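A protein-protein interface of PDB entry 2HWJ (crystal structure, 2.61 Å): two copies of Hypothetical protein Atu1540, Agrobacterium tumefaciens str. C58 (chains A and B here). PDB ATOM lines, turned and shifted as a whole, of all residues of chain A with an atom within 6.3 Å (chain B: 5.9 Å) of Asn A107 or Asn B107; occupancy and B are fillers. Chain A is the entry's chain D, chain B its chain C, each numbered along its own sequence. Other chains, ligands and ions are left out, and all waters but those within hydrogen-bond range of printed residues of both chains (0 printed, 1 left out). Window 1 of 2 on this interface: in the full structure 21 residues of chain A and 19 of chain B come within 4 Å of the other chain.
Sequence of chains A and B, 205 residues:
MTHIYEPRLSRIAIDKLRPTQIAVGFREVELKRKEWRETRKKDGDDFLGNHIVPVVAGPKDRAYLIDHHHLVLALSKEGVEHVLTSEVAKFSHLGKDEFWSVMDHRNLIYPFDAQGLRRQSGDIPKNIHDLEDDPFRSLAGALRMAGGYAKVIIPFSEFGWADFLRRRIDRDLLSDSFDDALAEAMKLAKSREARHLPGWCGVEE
ND2 of Asn A107 lies within hydrogen-bond range of OD1 of Asn B107, at 3.4 Å.
OD1 of Asn B107 lies close to O of Asp B104, at 3.3 Å.
Among the printed residues, pairs that only touch across the chains: His A105 with Phe B156.
Of chain B, only Asn B107 comes within 4 Å of Asn A107. Asn B107 touches just one residue of chain A: Asn A107 (3.4 Å). Of the printed residues of chain A, Phe B156 touches His A105 (3.7 Å). Of the printed residues of chain B, His A105 touches Phe B156 (3.7 Å). The nearest residue of chain B that does not touch Asn A107 is Asp B104 (5.6 Å). The nearest residue of chain A that does not touch Asn B107 is Pro A155 (5.9 Å). The nearest printed residue of chain B that does not touch His A105 is Pro B155 (5.2 Å).
Hydrophobic or aromatic side chains of chain A within 4 Å of the printed part of chain B: His A105. Of the 10 printed residues of chain B, 2 touch a printed residue of chain A. Printed residues of chain B that touch a printed residue of chain A: Asn B107 and Phe B156.
His A105 touches Phe B156, but with the chains exchanged Phe A156 does not touch His B105 (4.6 Å). Asn B107 touches its own counterpart, Asn A107.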
ATOM      1  N   VAL A 102     -20.668  11.037  24.528  1.00  0.00           N
ATOM      2  CA  VAL A 102     -20.458  10.469  25.864  1.00  0.00           C
ATOM      3  C   VAL A 102     -21.314   9.206  26.018  1.00  0.00           C
ATOM      4  O   VAL A 102     -20.878   8.210  26.654  1.00  0.00           O
ATOM      5  CB  VAL A 102     -20.919  11.442  26.973  1.00  0.00           C
ATOM      6  CG1 VAL A 102     -21.142  10.716  28.294  1.00  0.00           C
ATOM      7  CG2 VAL A 102     -20.004  12.573  27.143  1.00  0.00           C
ATOM      8  N   MET A 103     -22.541   9.255  25.474  1.00  0.00           N
ATOM      9  CA  MET A 103     -23.399   8.085  25.466  1.00  0.00           C
ATOM     10  C   MET A 103     -22.657   6.907  24.826  1.00  0.00           C
ATOM     11  O   MET A 103     -22.473   5.865  25.453  1.00  0.00           O
ATOM     12  CB  MET A 103     -24.690   8.366  24.728  1.00  0.00           C
ATOM     13  CG  MET A 103     -25.712   9.187  25.557  1.00  0.00           C
ATOM     14  SD  MET A 103     -26.279   8.364  27.304  1.00  0.00           S
ATOM     15  CE  MET A 103     -27.870   7.531  26.582  1.00  0.00           C
ATOM     16  N   ASP A 104     -22.188   7.093  23.591  1.00  0.00           N
ATOM     17  CA  ASP A 104     -21.427   6.058  22.879  1.00  0.00           C
ATOM     18  C   ASP A 104     -20.201   5.574  23.644  1.00  0.00           C
ATOM     19  O   ASP A 104     -19.747   4.464  23.472  1.00  0.00           O
ATOM     20  CB  ASP A 104     -21.005   6.630  21.540  1.00  0.00           C
ATOM     21  CG  ASP A 104     -20.513   5.584  20.571  1.00  0.00           C
ATOM     22  OD1 ASP A 104     -20.512   4.358  20.877  1.00  0.00           O
ATOM     23  OD2 ASP A 104     -20.153   6.014  19.451  1.00  0.00           O
ATOM     24  N   HIS A 105     -19.654   6.410  24.493  1.00  0.00           N
ATOM     25  CA  HIS A 105     -18.372   6.127  25.087  1.00  0.00           C
ATOM     26  C   HIS A 105     -18.644   5.257  26.272  1.00  0.00           C
ATOM     27  O   HIS A 105     -17.794   4.486  26.702  1.00  0.00           O
ATOM     28  CB  HIS A 105     -17.737   7.413  25.598  1.00  0.00           C
ATOM     29  CG  HIS A 105     -16.329   7.614  25.149  1.00  0.00           C
ATOM     30  ND1 HIS A 105     -16.000   8.449  24.100  1.00  0.00           N
ATOM     31  CD2 HIS A 105     -15.163   7.089  25.601  1.00  0.00           C
ATOM     32  CE1 HIS A 105     -14.696   8.400  23.896  1.00  0.00           C
ATOM     33  NE2 HIS A 105     -14.168   7.576  24.789  1.00  0.00           N
ATOM     34  N   ARG A 106     -19.831   5.412  26.829  1.00  0.00           N
ATOM     35  CA  ARG A 106     -20.163   4.659  28.010  1.00  0.00           C
ATOM     36  C   ARG A 106     -20.972   3.440  27.677  1.00  0.00           C
ATOM     37  O   ARG A 106     -21.428   2.757  28.566  1.00  0.00           O
ATOM     38  CB  ARG A 106     -20.873   5.537  29.025  1.00  0.00           C
ATOM     39  CG  ARG A 106     -19.860   6.141  29.926  1.00  0.00           C
ATOM     40  CD  ARG A 106     -20.278   7.529  30.219  1.00  0.00           C
ATOM     41  NE  ARG A 106     -21.072   7.593  31.437  1.00  0.00           N
ATOM     42  CZ  ARG A 106     -20.529   7.794  32.633  1.00  0.00           C
ATOM     43  NH1 ARG A 106     -19.198   7.922  32.747  1.00  0.00           N
ATOM     44  NH2 ARG A 106     -21.315   7.861  33.701  1.00  0.00           N
ATOM     45  N   ASN A 107     -21.103   3.180  26.379  1.00  0.00           N
ATOM     46  CA  ASN A 107     -21.942   2.113  25.812  1.00  0.00           C
ATOM     47  C   ASN A 107     -23.376   2.072  26.363  1.00  0.00           C
ATOM     48  O   ASN A 107     -23.870   1.023  26.818  1.00  0.00           O
ATOM     49  CB  ASN A 107     -21.203   0.765  25.855  1.00  0.00           C
ATOM     50  CG  ASN A 107     -19.951   0.769  24.942  1.00  0.00           C
ATOM     51  OD1 ASN A 107     -20.030   0.980  23.707  1.00  0.00           O
ATOM     52  ND2 ASN A 107     -18.811   0.582  25.542  1.00  0.00           N
ATOM     53  N   LEU A 108     -24.040   3.216  26.299  1.00  0.00           N
ATOM     54  CA  LEU A 108     -25.430   3.269  26.592  1.00  0.00           C
ATOM     55  C   LEU A 108     -26.291   3.457  25.323  1.00  0.00           C
ATOM     56  O   LEU A 108     -27.519   3.652  25.412  1.00  0.00           O
ATOM     57  CB  LEU A 108     -25.695   4.374  27.592  1.00  0.00           C
ATOM     58  CG  LEU A 108     -24.777   4.289  28.818  1.00  0.00           C
ATOM     59  CD1 LEU A 108     -24.824   5.612  29.630  1.00  0.00           C
ATOM     60  CD2 LEU A 108     -25.107   3.058  29.688  1.00  0.00           C
ATOM     61  N   ILE A 109     -25.695   3.431  24.132  1.00  0.00           N
ATOM     62  CA  ILE A 109     -26.516   3.459  22.935  1.00  0.00           C
ATOM     63  C   ILE A 109     -26.183   2.229  22.069  1.00  0.00           C
ATOM     64  O   ILE A 109     -25.097   1.673  22.190  1.00  0.00           O
ATOM     65  CB  ILE A 109     -26.392   4.798  22.178  1.00  0.00           C
ATOM     66  CG1 ILE A 109     -24.956   5.055  21.688  1.00  0.00           C
ATOM     67  CG2 ILE A 109     -26.789   5.941  23.069  1.00  0.00           C
ATOM     68  CD1 ILE A 109     -24.637   6.572  21.477  1.00  0.00           C
ATOM     69  N   PRO A 155     -22.721  -5.589  28.086  1.00  0.00           N
ATOM     70  CA  PRO A 155     -23.397  -4.796  27.081  1.00  0.00           C
ATOM     71  C   PRO A 155     -23.861  -5.498  25.779  1.00  0.00           C
ATOM     72  O   PRO A 155     -23.035  -5.970  24.984  1.00  0.00           O
ATOM     73  CB  PRO A 155     -22.337  -3.742  26.770  1.00  0.00           C
ATOM     74  CG  PRO A 155     -21.501  -3.656  28.141  1.00  0.00           C
ATOM     75  CD  PRO A 155     -22.046  -4.711  29.050  1.00  0.00           C
ATOM     76  N   PHE A 156     -25.186  -5.546  25.596  1.00  0.00           N
ATOM     77  CA  PHE A 156     -25.835  -6.003  24.382  1.00  0.00           C
ATOM     78  C   PHE A 156     -25.473  -7.391  23.897  1.00  0.00           C
ATOM     79  O   PHE A 156     -25.467  -7.618  22.699  1.00  0.00           O
ATOM     80  CB  PHE A 156     -25.609  -4.985  23.259  1.00  0.00           C
ATOM     81  CG  PHE A 156     -26.009  -3.598  23.647  1.00  0.00           C
ATOM     82  CD1 PHE A 156     -25.048  -2.659  24.040  1.00  0.00           C
ATOM     83  CD2 PHE A 156     -27.367  -3.235  23.689  1.00  0.00           C
ATOM     84  CE1 PHE A 156     -25.430  -1.375  24.432  1.00  0.00           C
ATOM     85  CE2 PHE A 156     -27.746  -1.932  24.098  1.00  0.00           C
ATOM     86  CZ  PHE A 156     -26.779  -1.014  24.467  1.00  0.00           C
ATOM     87  N   VAL B 102     -17.166  -8.164  15.759  1.00  0.00           N
ATOM     88  CA  VAL B 102     -16.945  -8.722  17.054  1.00  0.00           C
ATOM     89  C   VAL B 102     -16.072  -7.726  17.798  1.00  0.00           C
ATOM     90  O   VAL B 102     -16.397  -7.298  18.929  1.00  0.00           O
ATOM     91  CB  VAL B 102     -16.425 -10.220  17.004  1.00  0.00           C
ATOM     92  CG1 VAL B 102     -15.775 -10.636  18.251  1.00  0.00           C
ATOM     93  CG2 VAL B 102     -17.576 -11.098  16.802  1.00  0.00           C
ATOM     94  N   MET B 103     -14.996  -7.310  17.153  1.00  0.00           N
ATOM     95  CA  MET B 103     -14.064  -6.386  17.809  1.00  0.00           C
ATOM     96  C   MET B 103     -14.742  -5.200  18.455  1.00  0.00           C
ATOM     97  O   MET B 103     -14.444  -4.861  19.590  1.00  0.00           O
ATOM     98  CB  MET B 103     -13.022  -5.918  16.837  1.00  0.00           C
ATOM     99  CG  MET B 103     -12.146  -7.029  16.360  1.00  0.00           C
ATOM    100  SD  MET B 103     -11.049  -7.543  17.846  1.00  0.00           S
ATOM    101  CE  MET B 103      -9.342  -6.692  17.400  1.00  0.00           C
ATOM    102  N   ASP B 104     -15.667  -4.574  17.748  1.00  0.00           N
ATOM    103  CA  ASP B 104     -16.351  -3.420  18.320  1.00  0.00           C
ATOM    104  C   ASP B 104     -17.286  -3.823  19.473  1.00  0.00           C
ATOM    105  O   ASP B 104     -17.235  -3.207  20.555  1.00  0.00           O
ATOM    106  CB  ASP B 104     -17.130  -2.689  17.251  1.00  0.00           C
ATOM    107  CG  ASP B 104     -18.130  -1.714  17.837  1.00  0.00           C
ATOM    108  OD1 ASP B 104     -18.204  -1.557  19.099  1.00  0.00           O
ATOM    109  OD2 ASP B 104     -18.866  -1.101  17.017  1.00  0.00           O
ATOM    110  N   HIS B 105     -18.142  -4.840  19.236  1.00  0.00           N
ATOM    111  CA  HIS B 105     -19.060  -5.369  20.258  1.00  0.00           C
ATOM    112  C   HIS B 105     -18.272  -5.535  21.576  1.00  0.00           C
ATOM    113  O   HIS B 105     -18.829  -5.361  22.664  1.00  0.00           O
ATOM    114  CB  HIS B 105     -19.748  -6.696  19.782  1.00  0.00           C
ATOM    115  CG  HIS B 105     -21.080  -6.516  19.081  1.00  0.00           C
ATOM    116  ND1 HIS B 105     -21.226  -5.831  17.888  1.00  0.00           N
ATOM    117  CD2 HIS B 105     -22.318  -6.970  19.399  1.00  0.00           C
ATOM    118  CE1 HIS B 105     -22.497  -5.840  17.523  1.00  0.00           C
ATOM    119  NE2 HIS B 105     -23.179  -6.537  18.417  1.00  0.00           N
ATOM    120  N   ARG B 106     -16.974  -5.819  21.463  1.00  0.00           N
ATOM    121  CA  ARG B 106     -16.133  -5.948  22.663  1.00  0.00           C
ATOM    122  C   ARG B 106     -15.264  -4.737  23.077  1.00  0.00           C
ATOM    123  O   ARG B 106     -14.566  -4.771  24.089  1.00  0.00           O
ATOM    124  CB  ARG B 106     -15.287  -7.194  22.558  1.00  0.00           C
ATOM    125  CG  ARG B 106     -16.090  -8.362  22.267  1.00  0.00           C
ATOM    126  CD  ARG B 106     -15.326  -9.533  22.640  1.00  0.00           C
ATOM    127  NE  ARG B 106     -16.007 -10.261  23.684  1.00  0.00           N
ATOM    128  CZ  ARG B 106     -15.768 -11.537  23.972  1.00  0.00           C
ATOM    129  NH1 ARG B 106     -14.856 -12.217  23.275  1.00  0.00           N
ATOM    130  NH2 ARG B 106     -16.452 -12.139  24.951  1.00  0.00           N
ATOM    131  N   ASN B 107     -15.332  -3.668  22.287  1.00  0.00           N
ATOM    132  CA  ASN B 107     -14.513  -2.463  22.465  1.00  0.00           C
ATOM    133  C   ASN B 107     -13.061  -2.766  22.465  1.00  0.00           C
ATOM    134  O   ASN B 107     -12.296  -2.241  23.308  1.00  0.00           O
ATOM    135  CB  ASN B 107     -14.825  -1.762  23.763  1.00  0.00           C
ATOM    136  CG  ASN B 107     -16.285  -1.691  24.028  1.00  0.00           C
ATOM    137  OD1 ASN B 107     -17.125  -1.222  23.198  1.00  0.00           O
ATOM    138  ND2 ASN B 107     -16.628  -2.157  25.217  1.00  0.00           N
ATOM    139  N   LEU B 108     -12.672  -3.639  21.565  1.00  0.00           N
ATOM    140  CA  LEU B 108     -11.252  -3.781  21.372  1.00  0.00           C
ATOM    141  C   LEU B 108     -10.736  -2.804  20.326  1.00  0.00           C
ATOM    142  O   LEU B 108      -9.545  -2.752  20.054  1.00  0.00           O
ATOM    143  CB  LEU B 108     -10.890  -5.240  21.062  1.00  0.00           C
ATOM    144  CG  LEU B 108     -11.219  -6.038  22.339  1.00  0.00           C
ATOM    145  CD1 LEU B 108     -11.270  -7.438  21.982  1.00  0.00           C
ATOM    146  CD2 LEU B 108     -10.251  -5.751  23.534  1.00  0.00           C
ATOM    147  N   ILE B 109     -11.646  -2.038  19.728  1.00  0.00           N
ATOM    148  CA  ILE B 109     -11.255  -1.092  18.716  1.00  0.00           C
ATOM    149  C   ILE B 109     -11.670   0.298  19.138  1.00  0.00           C
ATOM    150  O   ILE B 109     -12.465   0.439  20.061  1.00  0.00           O
ATOM    151  CB  ILE B 109     -11.847  -1.420  17.361  1.00  0.00           C
ATOM    152  CG1 ILE B 109     -13.365  -1.298  17.402  1.00  0.00           C
ATOM    153  CG2 ILE B 109     -11.369  -2.767  16.890  1.00  0.00           C
ATOM    154  CD1 ILE B 109     -13.990  -1.394  16.033  1.00  0.00           C
ATOM    155  N   PRO B 155     -12.100   1.077  29.492  1.00  0.00           N
ATOM    156  CA  PRO B 155     -11.292   1.312  28.246  1.00  0.00           C
ATOM    157  C   PRO B 155     -11.418   2.772  27.782  1.00  0.00           C
ATOM    158  O   PRO B 155     -12.509   3.295  27.866  1.00  0.00           O
ATOM    159  CB  PRO B 155     -12.042   0.464  27.185  1.00  0.00           C
ATOM    160  CG  PRO B 155     -13.494   0.188  27.831  1.00  0.00           C
ATOM    161  CD  PRO B 155     -13.135   0.035  29.327  1.00  0.00           C
ATOM    162  N   PHE B 156     -10.339   3.423  27.298  1.00  0.00           N
ATOM    163  CA  PHE B 156     -10.479   4.682  26.540  1.00  0.00           C
ATOM    164  C   PHE B 156     -10.887   5.872  27.404  1.00  0.00           C
ATOM    165  O   PHE B 156     -11.273   6.894  26.964  1.00  0.00           O
ATOM    166  CB  PHE B 156     -11.449   4.468  25.337  1.00  0.00           C
ATOM    167  CG  PHE B 156     -11.035   3.310  24.429  1.00  0.00           C
ATOM    168  CD1 PHE B 156     -11.891   2.240  24.205  1.00  0.00           C
ATOM    169  CD2 PHE B 156      -9.739   3.280  23.845  1.00  0.00           C
ATOM    170  CE1 PHE B 156     -11.469   1.134  23.362  1.00  0.00           C
ATOM    171  CE2 PHE B 156      -9.288   2.183  23.058  1.00  0.00           C
ATOM    172  CZ  PHE B 156     -10.141   1.100  22.795  1.00  0.00           C
